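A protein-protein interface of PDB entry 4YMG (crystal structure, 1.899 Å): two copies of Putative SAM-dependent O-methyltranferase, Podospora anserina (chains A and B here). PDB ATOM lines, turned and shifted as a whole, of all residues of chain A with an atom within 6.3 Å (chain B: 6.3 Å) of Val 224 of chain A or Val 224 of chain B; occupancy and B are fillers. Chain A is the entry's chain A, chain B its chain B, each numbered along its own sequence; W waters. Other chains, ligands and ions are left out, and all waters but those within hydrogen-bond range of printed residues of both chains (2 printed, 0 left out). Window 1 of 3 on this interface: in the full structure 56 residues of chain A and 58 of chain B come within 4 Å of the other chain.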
ATOM      1  N   SER A   4       1.485  27.574  26.230  1.00  0.00           N
ATOM      2  CA  SER A   4       0.514  27.071  25.270  1.00  0.00           C
ATOM      3  C   SER A   4       0.527  25.559  25.202  1.00  0.00           C
ATOM      4  O   SER A   4      -0.077  24.967  24.305  1.00  0.00           O
ATOM      5  CB  SER A   4       0.796  27.631  23.873  1.00  0.00           C
ATOM      6  OG  SER A   4       0.680  29.038  23.854  1.00  0.00           O
ATOM      7  N   TRP A  56      -6.255  13.192  11.772  1.00  0.00           N
ATOM      8  CA  TRP A  56      -5.995  14.601  11.517  1.00  0.00           C
ATOM      9  C   TRP A  56      -5.769  14.842  10.024  1.00  0.00           C
ATOM     10  O   TRP A  56      -6.308  15.796   9.464  1.00  0.00           O
ATOM     11  CB  TRP A  56      -4.802  15.082  12.342  1.00  0.00           C
ATOM     12  CG  TRP A  56      -4.223  16.399  11.912  1.00  0.00           C
ATOM     13  CD1 TRP A  56      -4.778  17.639  12.070  1.00  0.00           C
ATOM     14  CD2 TRP A  56      -2.954  16.605  11.283  1.00  0.00           C
ATOM     15  NE1 TRP A  56      -3.935  18.605  11.561  1.00  0.00           N
ATOM     16  CE2 TRP A  56      -2.809  17.993  11.075  1.00  0.00           C
ATOM     17  CE3 TRP A  56      -1.924  15.747  10.873  1.00  0.00           C
ATOM     18  CZ2 TRP A  56      -1.675  18.545  10.465  1.00  0.00           C
ATOM     19  CZ3 TRP A  56      -0.801  16.296  10.269  1.00  0.00           C
ATOM     20  CH2 TRP A  56      -0.683  17.682  10.083  1.00  0.00           C
ATOM     21  N   ASP A 172       6.252  18.172   9.394  1.00  0.00           N
ATOM     22  CA  ASP A 172       6.009  17.273  10.515  1.00  0.00           C
ATOM     23  C   ASP A 172       7.270  17.069  11.334  1.00  0.00           C
ATOM     24  O   ASP A 172       8.384  17.233  10.813  1.00  0.00           O
ATOM     25  CB  ASP A 172       5.510  15.917  10.008  1.00  0.00           C
ATOM     26  CG  ASP A 172       4.684  15.170  11.038  1.00  0.00           C
ATOM     27  OD1 ASP A 172       3.956  15.838  11.803  1.00  0.00           O
ATOM     28  OD2 ASP A 172       4.754  13.917  11.074  1.00  0.00           O
ATOM     29  N   PHE A 175       9.735  19.424  16.174  1.00  0.00           N
ATOM     30  CA  PHE A 175      10.303  19.465  17.534  1.00  0.00           C
ATOM     31  C   PHE A 175      11.430  18.449  17.778  1.00  0.00           C
ATOM     32  O   PHE A 175      12.176  18.579  18.745  1.00  0.00           O
ATOM     33  CB  PHE A 175       9.222  19.214  18.587  1.00  0.00           C
ATOM     34  CG  PHE A 175       8.248  20.353  18.779  1.00  0.00           C
ATOM     35  CD1 PHE A 175       8.484  21.604  18.240  1.00  0.00           C
ATOM     36  CD2 PHE A 175       7.095  20.160  19.524  1.00  0.00           C
ATOM     37  CE1 PHE A 175       7.578  22.641  18.426  1.00  0.00           C
ATOM     38  CE2 PHE A 175       6.191  21.194  19.723  1.00  0.00           C
ATOM     39  CZ  PHE A 175       6.434  22.429  19.177  1.00  0.00           C
ATOM     40  N   LEU A 222       3.123  25.189  15.246  1.00  0.00           N
ATOM     41  CA  LEU A 222       2.039  24.703  16.097  1.00  0.00           C
ATOM     42  C   LEU A 222       2.511  23.577  17.019  1.00  0.00           C
ATOM     43  O   LEU A 222       3.014  22.542  16.549  1.00  0.00           O
ATOM     44  CB  LEU A 222       0.886  24.220  15.212  1.00  0.00           C
ATOM     45  CG  LEU A 222      -0.526  24.128  15.775  1.00  0.00           C
ATOM     46  CD1 LEU A 222      -1.017  25.524  16.141  1.00  0.00           C
ATOM     47  CD2 LEU A 222      -1.439  23.466  14.757  1.00  0.00           C
ATOM     48  N   PRO A 223       2.332  23.755  18.337  1.00  0.00           N
ATOM     49  CA  PRO A 223       2.780  22.741  19.292  1.00  0.00           C
ATOM     50  C   PRO A 223       1.812  21.566  19.402  1.00  0.00           C
ATOM     51  O   PRO A 223       1.235  21.332  20.466  1.00  0.00           O
ATOM     52  CB  PRO A 223       2.838  23.511  20.607  1.00  0.00           C
ATOM     53  CG  PRO A 223       1.741  24.526  20.462  1.00  0.00           C
ATOM     54  CD  PRO A 223       1.775  24.943  19.017  1.00  0.00           C
ATOM     55  N   VAL A 224       1.655  20.824  18.320  1.00  0.00           N
ATOM     56  CA  VAL A 224       0.805  19.645  18.335  1.00  0.00           C
ATOM     57  C   VAL A 224       1.633  18.483  17.798  1.00  0.00           C
ATOM     58  O   VAL A 224       2.532  18.687  16.969  1.00  0.00           O
ATOM     59  CB  VAL A 224      -0.482  19.851  17.491  1.00  0.00           C
ATOM     60  CG1 VAL A 224      -0.143  19.977  16.005  1.00  0.00           C
ATOM     61  CG2 VAL A 224      -1.518  18.717  17.731  1.00  0.00           C
ATOM     62  N   PHE A 225       1.327  17.281  18.279  1.00  0.00           N
ATOM     63  CA  PHE A 225       2.048  16.067  17.911  1.00  0.00           C
ATOM     64  C   PHE A 225       3.535  16.298  18.186  1.00  0.00           C
ATOM     65  O   PHE A 225       3.895  16.678  19.295  1.00  0.00           O
ATOM     66  CB  PHE A 225       1.784  15.682  16.447  1.00  0.00           C
ATOM     67  CG  PHE A 225       0.310  15.519  16.117  1.00  0.00           C
ATOM     68  CD1 PHE A 225      -0.519  14.768  16.941  1.00  0.00           C
ATOM     69  CD2 PHE A 225      -0.238  16.121  14.987  1.00  0.00           C
ATOM     70  CE1 PHE A 225      -1.882  14.618  16.645  1.00  0.00           C
ATOM     71  CE2 PHE A 225      -1.598  15.981  14.684  1.00  0.00           C
ATOM     72  CZ  PHE A 225      -2.414  15.224  15.512  1.00  0.00           C
ATOM     73  N   ASP A 226       4.385  16.089  17.187  1.00  0.00           N
ATOM     74  CA  ASP A 226       5.837  16.274  17.380  1.00  0.00           C
ATOM     75  C   ASP A 226       6.271  17.610  16.778  1.00  0.00           C
ATOM     76  O   ASP A 226       7.421  17.783  16.355  1.00  0.00           O
ATOM     77  CB  ASP A 226       6.612  15.094  16.768  1.00  0.00           C
ATOM     78  CG  ASP A 226       8.098  15.080  17.157  1.00  0.00           C
ATOM     79  OD1 ASP A 226       8.453  15.668  18.194  1.00  0.00           O
ATOM     80  OD2 ASP A 226       8.914  14.488  16.412  1.00  0.00           O
ATOM     81  N   GLY A 227       5.329  18.558  16.747  1.00  0.00           N
ATOM     82  CA  GLY A 227       5.573  19.882  16.205  1.00  0.00           C
ATOM     83  C   GLY A 227       5.182  19.953  14.737  1.00  0.00           C
ATOM     84  O   GLY A 227       5.693  19.207  13.907  1.00  0.00           O
ATOM     85  N   VAL A 228       4.257  20.841  14.404  1.00  0.00           N
ATOM     86  CA  VAL A 228       3.910  21.026  13.000  1.00  0.00           C
ATOM     87  C   VAL A 228       4.078  22.478  12.582  1.00  0.00           C
ATOM     88  O   VAL A 228       3.447  23.379  13.133  1.00  0.00           O
ATOM     89  CB  VAL A 228       2.469  20.571  12.710  1.00  0.00           C
ATOM     90  CG1 VAL A 228       2.120  20.803  11.231  1.00  0.00           C
ATOM     91  CG2 VAL A 228       2.304  19.106  13.071  1.00  0.00           C
ATOM     92  N   SER B   4       0.357  10.217  20.535  1.00  0.00           N
ATOM     93  CA  SER B   4       0.710  11.298  19.634  1.00  0.00           C
ATOM     94  C   SER B   4       1.154  12.557  20.363  1.00  0.00           C
ATOM     95  O   SER B   4       1.332  13.591  19.729  1.00  0.00           O
ATOM     96  CB  SER B   4      -0.481  11.647  18.738  1.00  0.00           C
ATOM     97  OG  SER B   4      -1.052  10.490  18.164  1.00  0.00           O
ATOM     98  N   TRP B  56      -2.034  31.821  16.120  1.00  0.00           N
ATOM     99  CA  TRP B  56      -2.760  30.725  15.482  1.00  0.00           C
ATOM    100  C   TRP B  56      -4.099  31.206  14.935  1.00  0.00           C
ATOM    101  O   TRP B  56      -4.508  30.805  13.847  1.00  0.00           O
ATOM    102  CB  TRP B  56      -2.953  29.577  16.474  1.00  0.00           C
ATOM    103  CG  TRP B  56      -3.998  28.555  16.096  1.00  0.00           C
ATOM    104  CD1 TRP B  56      -3.888  27.570  15.149  1.00  0.00           C
ATOM    105  CD2 TRP B  56      -5.293  28.411  16.675  1.00  0.00           C
ATOM    106  NE1 TRP B  56      -5.039  26.822  15.111  1.00  0.00           N
ATOM    107  CE2 TRP B  56      -5.919  27.317  16.035  1.00  0.00           C
ATOM    108  CE3 TRP B  56      -5.992  29.103  17.670  1.00  0.00           C
ATOM    109  CZ2 TRP B  56      -7.206  26.900  16.358  1.00  0.00           C
ATOM    110  CZ3 TRP B  56      -7.272  28.687  17.991  1.00  0.00           C
ATOM    111  CH2 TRP B  56      -7.866  27.592  17.340  1.00  0.00           C
ATOM    112  N   ASP B 172     -12.599  25.611  22.192  1.00  0.00           N
ATOM    113  CA  ASP B 172     -11.347  25.822  22.939  1.00  0.00           C
ATOM    114  C   ASP B 172     -11.414  25.181  24.334  1.00  0.00           C
ATOM    115  O   ASP B 172     -12.505  24.954  24.858  1.00  0.00           O
ATOM    116  CB  ASP B 172     -11.065  27.330  23.047  1.00  0.00           C
ATOM    117  CG  ASP B 172      -9.605  27.639  23.288  1.00  0.00           C
ATOM    118  OD1 ASP B 172      -8.753  26.921  22.738  1.00  0.00           O
ATOM    119  OD2 ASP B 172      -9.317  28.598  24.034  1.00  0.00           O
ATOM    120  N   PHE B 175      -9.821  20.054  26.866  1.00  0.00           N
ATOM    121  CA  PHE B 175      -9.128  19.190  27.831  1.00  0.00           C
ATOM    122  C   PHE B 175      -9.347  19.580  29.300  1.00  0.00           C
ATOM    123  O   PHE B 175      -9.080  18.779  30.190  1.00  0.00           O
ATOM    124  CB  PHE B 175      -7.620  19.200  27.569  1.00  0.00           C
ATOM    125  CG  PHE B 175      -7.189  18.424  26.355  1.00  0.00           C
ATOM    126  CD1 PHE B 175      -8.059  17.574  25.692  1.00  0.00           C
ATOM    127  CD2 PHE B 175      -5.874  18.517  25.901  1.00  0.00           C
ATOM    128  CE1 PHE B 175      -7.637  16.855  24.582  1.00  0.00           C
ATOM    129  CE2 PHE B 175      -5.446  17.800  24.795  1.00  0.00           C
ATOM    130  CZ  PHE B 175      -6.341  16.965  24.133  1.00  0.00           C
ATOM    131  N   LEU B 222      -8.068  17.747  18.608  1.00  0.00           N
ATOM    132  CA  LEU B 222      -6.634  17.938  18.413  1.00  0.00           C
ATOM    133  C   LEU B 222      -5.939  18.273  19.733  1.00  0.00           C
ATOM    134  O   LEU B 222      -6.369  19.177  20.445  1.00  0.00           O
ATOM    135  CB  LEU B 222      -6.398  19.048  17.382  1.00  0.00           C
ATOM    136  CG  LEU B 222      -5.177  18.927  16.464  1.00  0.00           C
ATOM    137  CD1 LEU B 222      -5.233  17.628  15.667  1.00  0.00           C
ATOM    138  CD2 LEU B 222      -5.112  20.128  15.532  1.00  0.00           C
ATOM    139  N   PRO B 223      -4.849  17.552  20.067  1.00  0.00           N
ATOM    140  CA  PRO B 223      -4.191  17.810  21.349  1.00  0.00           C
ATOM    141  C   PRO B 223      -3.214  18.978  21.257  1.00  0.00           C
ATOM    142  O   PRO B 223      -1.995  18.822  21.437  1.00  0.00           O
ATOM    143  CB  PRO B 223      -3.462  16.498  21.631  1.00  0.00           C
ATOM    144  CG  PRO B 223      -3.094  15.996  20.259  1.00  0.00           C
ATOM    145  CD  PRO B 223      -4.214  16.441  19.331  1.00  0.00           C
ATOM    146  N   VAL B 224      -3.757  20.152  20.969  1.00  0.00           N
ATOM    147  CA  VAL B 224      -2.960  21.370  20.904  1.00  0.00           C
ATOM    148  C   VAL B 224      -3.533  22.372  21.908  1.00  0.00           C
ATOM    149  O   VAL B 224      -4.737  22.346  22.179  1.00  0.00           O
ATOM    150  CB  VAL B 224      -2.947  21.957  19.478  1.00  0.00           C
ATOM    151  CG1 VAL B 224      -4.356  22.355  19.025  1.00  0.00           C
ATOM    152  CG2 VAL B 224      -1.963  23.145  19.380  1.00  0.00           C
ATOM    153  N   PHE B 225      -2.671  23.231  22.460  1.00  0.00           N
ATOM    154  CA  PHE B 225      -3.075  24.208  23.475  1.00  0.00           C
ATOM    155  C   PHE B 225      -3.776  23.479  24.629  1.00  0.00           C
ATOM    156  O   PHE B 225      -3.193  22.568  25.205  1.00  0.00           O
ATOM    157  CB  PHE B 225      -3.950  25.293  22.844  1.00  0.00           C
ATOM    158  CG  PHE B 225      -3.270  26.015  21.698  1.00  0.00           C
ATOM    159  CD1 PHE B 225      -1.988  26.522  21.848  1.00  0.00           C
ATOM    160  CD2 PHE B 225      -3.890  26.145  20.467  1.00  0.00           C
ATOM    161  CE1 PHE B 225      -1.346  27.178  20.792  1.00  0.00           C
ATOM    162  CE2 PHE B 225      -3.251  26.796  19.410  1.00  0.00           C
ATOM    163  CZ  PHE B 225      -1.974  27.308  19.582  1.00  0.00           C
ATOM    164  N   ASP B 226      -5.019  23.842  24.944  1.00  0.00           N
ATOM    165  CA  ASP B 226      -5.744  23.164  26.018  1.00  0.00           C
ATOM    166  C   ASP B 226      -6.819  22.234  25.422  1.00  0.00           C
ATOM    167  O   ASP B 226      -7.869  22.029  26.018  1.00  0.00           O
ATOM    168  CB  ASP B 226      -6.374  24.190  26.979  1.00  0.00           C
ATOM    169  CG  ASP B 226      -6.919  23.551  28.267  1.00  0.00           C
ATOM    170  OD1 ASP B 226      -6.468  22.444  28.632  1.00  0.00           O
ATOM    171  OD2 ASP B 226      -7.799  24.163  28.917  1.00  0.00           O
ATOM    172  N   GLY B 227      -6.527  21.682  24.249  1.00  0.00           N
ATOM    173  CA  GLY B 227      -7.446  20.809  23.534  1.00  0.00           C
ATOM    174  C   GLY B 227      -8.380  21.615  22.650  1.00  0.00           C
ATOM    175  O   GLY B 227      -9.078  22.496  23.138  1.00  0.00           O
ATOM    176  N   VAL B 228      -8.383  21.316  21.356  1.00  0.00           N
ATOM    177  CA  VAL B 228      -9.221  22.033  20.392  1.00  0.00           C
ATOM    178  C   VAL B 228     -10.032  21.046  19.559  1.00  0.00           C
ATOM    179  O   VAL B 228      -9.479  20.280  18.779  1.00  0.00           O
ATOM    180  CB  VAL B 228      -8.391  22.913  19.440  1.00  0.00           C
ATOM    181  CG1 VAL B 228      -9.292  23.555  18.382  1.00  0.00           C
ATOM    182  CG2 VAL B 228      -7.634  23.987  20.222  1.00  0.00           C
HETATM  183  O   HOH W   1      -0.006  22.385  22.701  1.00  0.00           O
HETATM  184  O   HOH W   2       0.096  16.962  20.917  1.00  0.00           O
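Phe 175 of chain A touches none of the printed residues of chain B.
Printed residues of chain B within 4 Å of Leu 222 of chain A: Trp 56 and Phe 225.
Of the printed residues of chain A, Pro 223 of chain B touches Val 224 and Phe 225.
The nearest residue of chain B that does not touch Val 224 of chain A is Ser 4 of chain B (5.3 Å).
Water W1 lies within hydrogen-bond range of the backbone carbonyl oxygen (O) of Pro 223 of chain A (2.8 Å), the backbone NH (N) of Phe 225 of chain B (2.8 Å) and the backbone carbonyl oxygen (O) of Ser 4 of chain A (3.0 Å).
Water W2 bridges O of Pro 223 of chain B (2.8 Å) and N of Phe 225 of chain A (2.9 Å).
Trp 56 of chain A touches Leu 222 of chain B, and with the chains exchanged Leu 222 of chain A touches Trp 56 of chain B.
Leu 222 of chain A touches Phe 225 of chain B, and with the chains exchanged Phe 225 of chain A touches Leu 222 of chain B.
Pro 223 of chain A touches Val 224 of chain B, and with the chains exchanged Val 224 of chain A touches Pro 223 of chain B.
Val 224 of chain A touches its own counterpart, Val 224 of chain B.
Positions printed for both chains: 4, 56, 172, 175, 222, 223, 224, 225, 226, 227 and 228.
Of the 11 pairs that touch across the chains among the printed residues, 9 have their exchanged pair printed and touching as well.
Ser 4 of chain A touches Phe 225 of chain B.
Trp 56 of chain A touches Leu 222 of chain B (CD1 to CD1, 3.6 Å).
Trp 56 of chain B touches Leu 222 of chain A.
CZ of Phe 225 of chain B touches CD1 of Leu 222 of chain A, at 3.99 Å.
O of Pro 223 of chain A touches CG2 of Val 224 of chain B, at 3.8 Å.
CG of Leu 222 of chain B touches CG2 of Val 224 of chain A, at 3.9 Å.
Val 224 of chain A touches Pro 223 of chain B (CG2 to O, 3.7 Å).
Val 224 of chain B touches Val 224 of chain A (CB to CB, 3.8 Å).
Ser 4 of chain B touches Phe 225 of chain A.
Pro 223 of chain B touches Phe 225 of chain A (CD to CE1, 3.997 Å).
Hydrophobic or aromatic side chains of chain A that line the printed part of chain B: Trp 56, Leu 222, Val 224 and Phe 225.
Among the printed residues, no Asp or Glu carboxylate lies within 4 Å of a Lys or Arg side-chain nitrogen of the other chain.
The backbone NH of Leu 222 of chain A lies within hydrogen-bond range of the backbone carbonyl oxygen of Val 228 of chain A (2.8 Å).
O of Val 228 of chain B lies within hydrogen-bond range of N of Leu 222 of chain B (2.9 Å).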
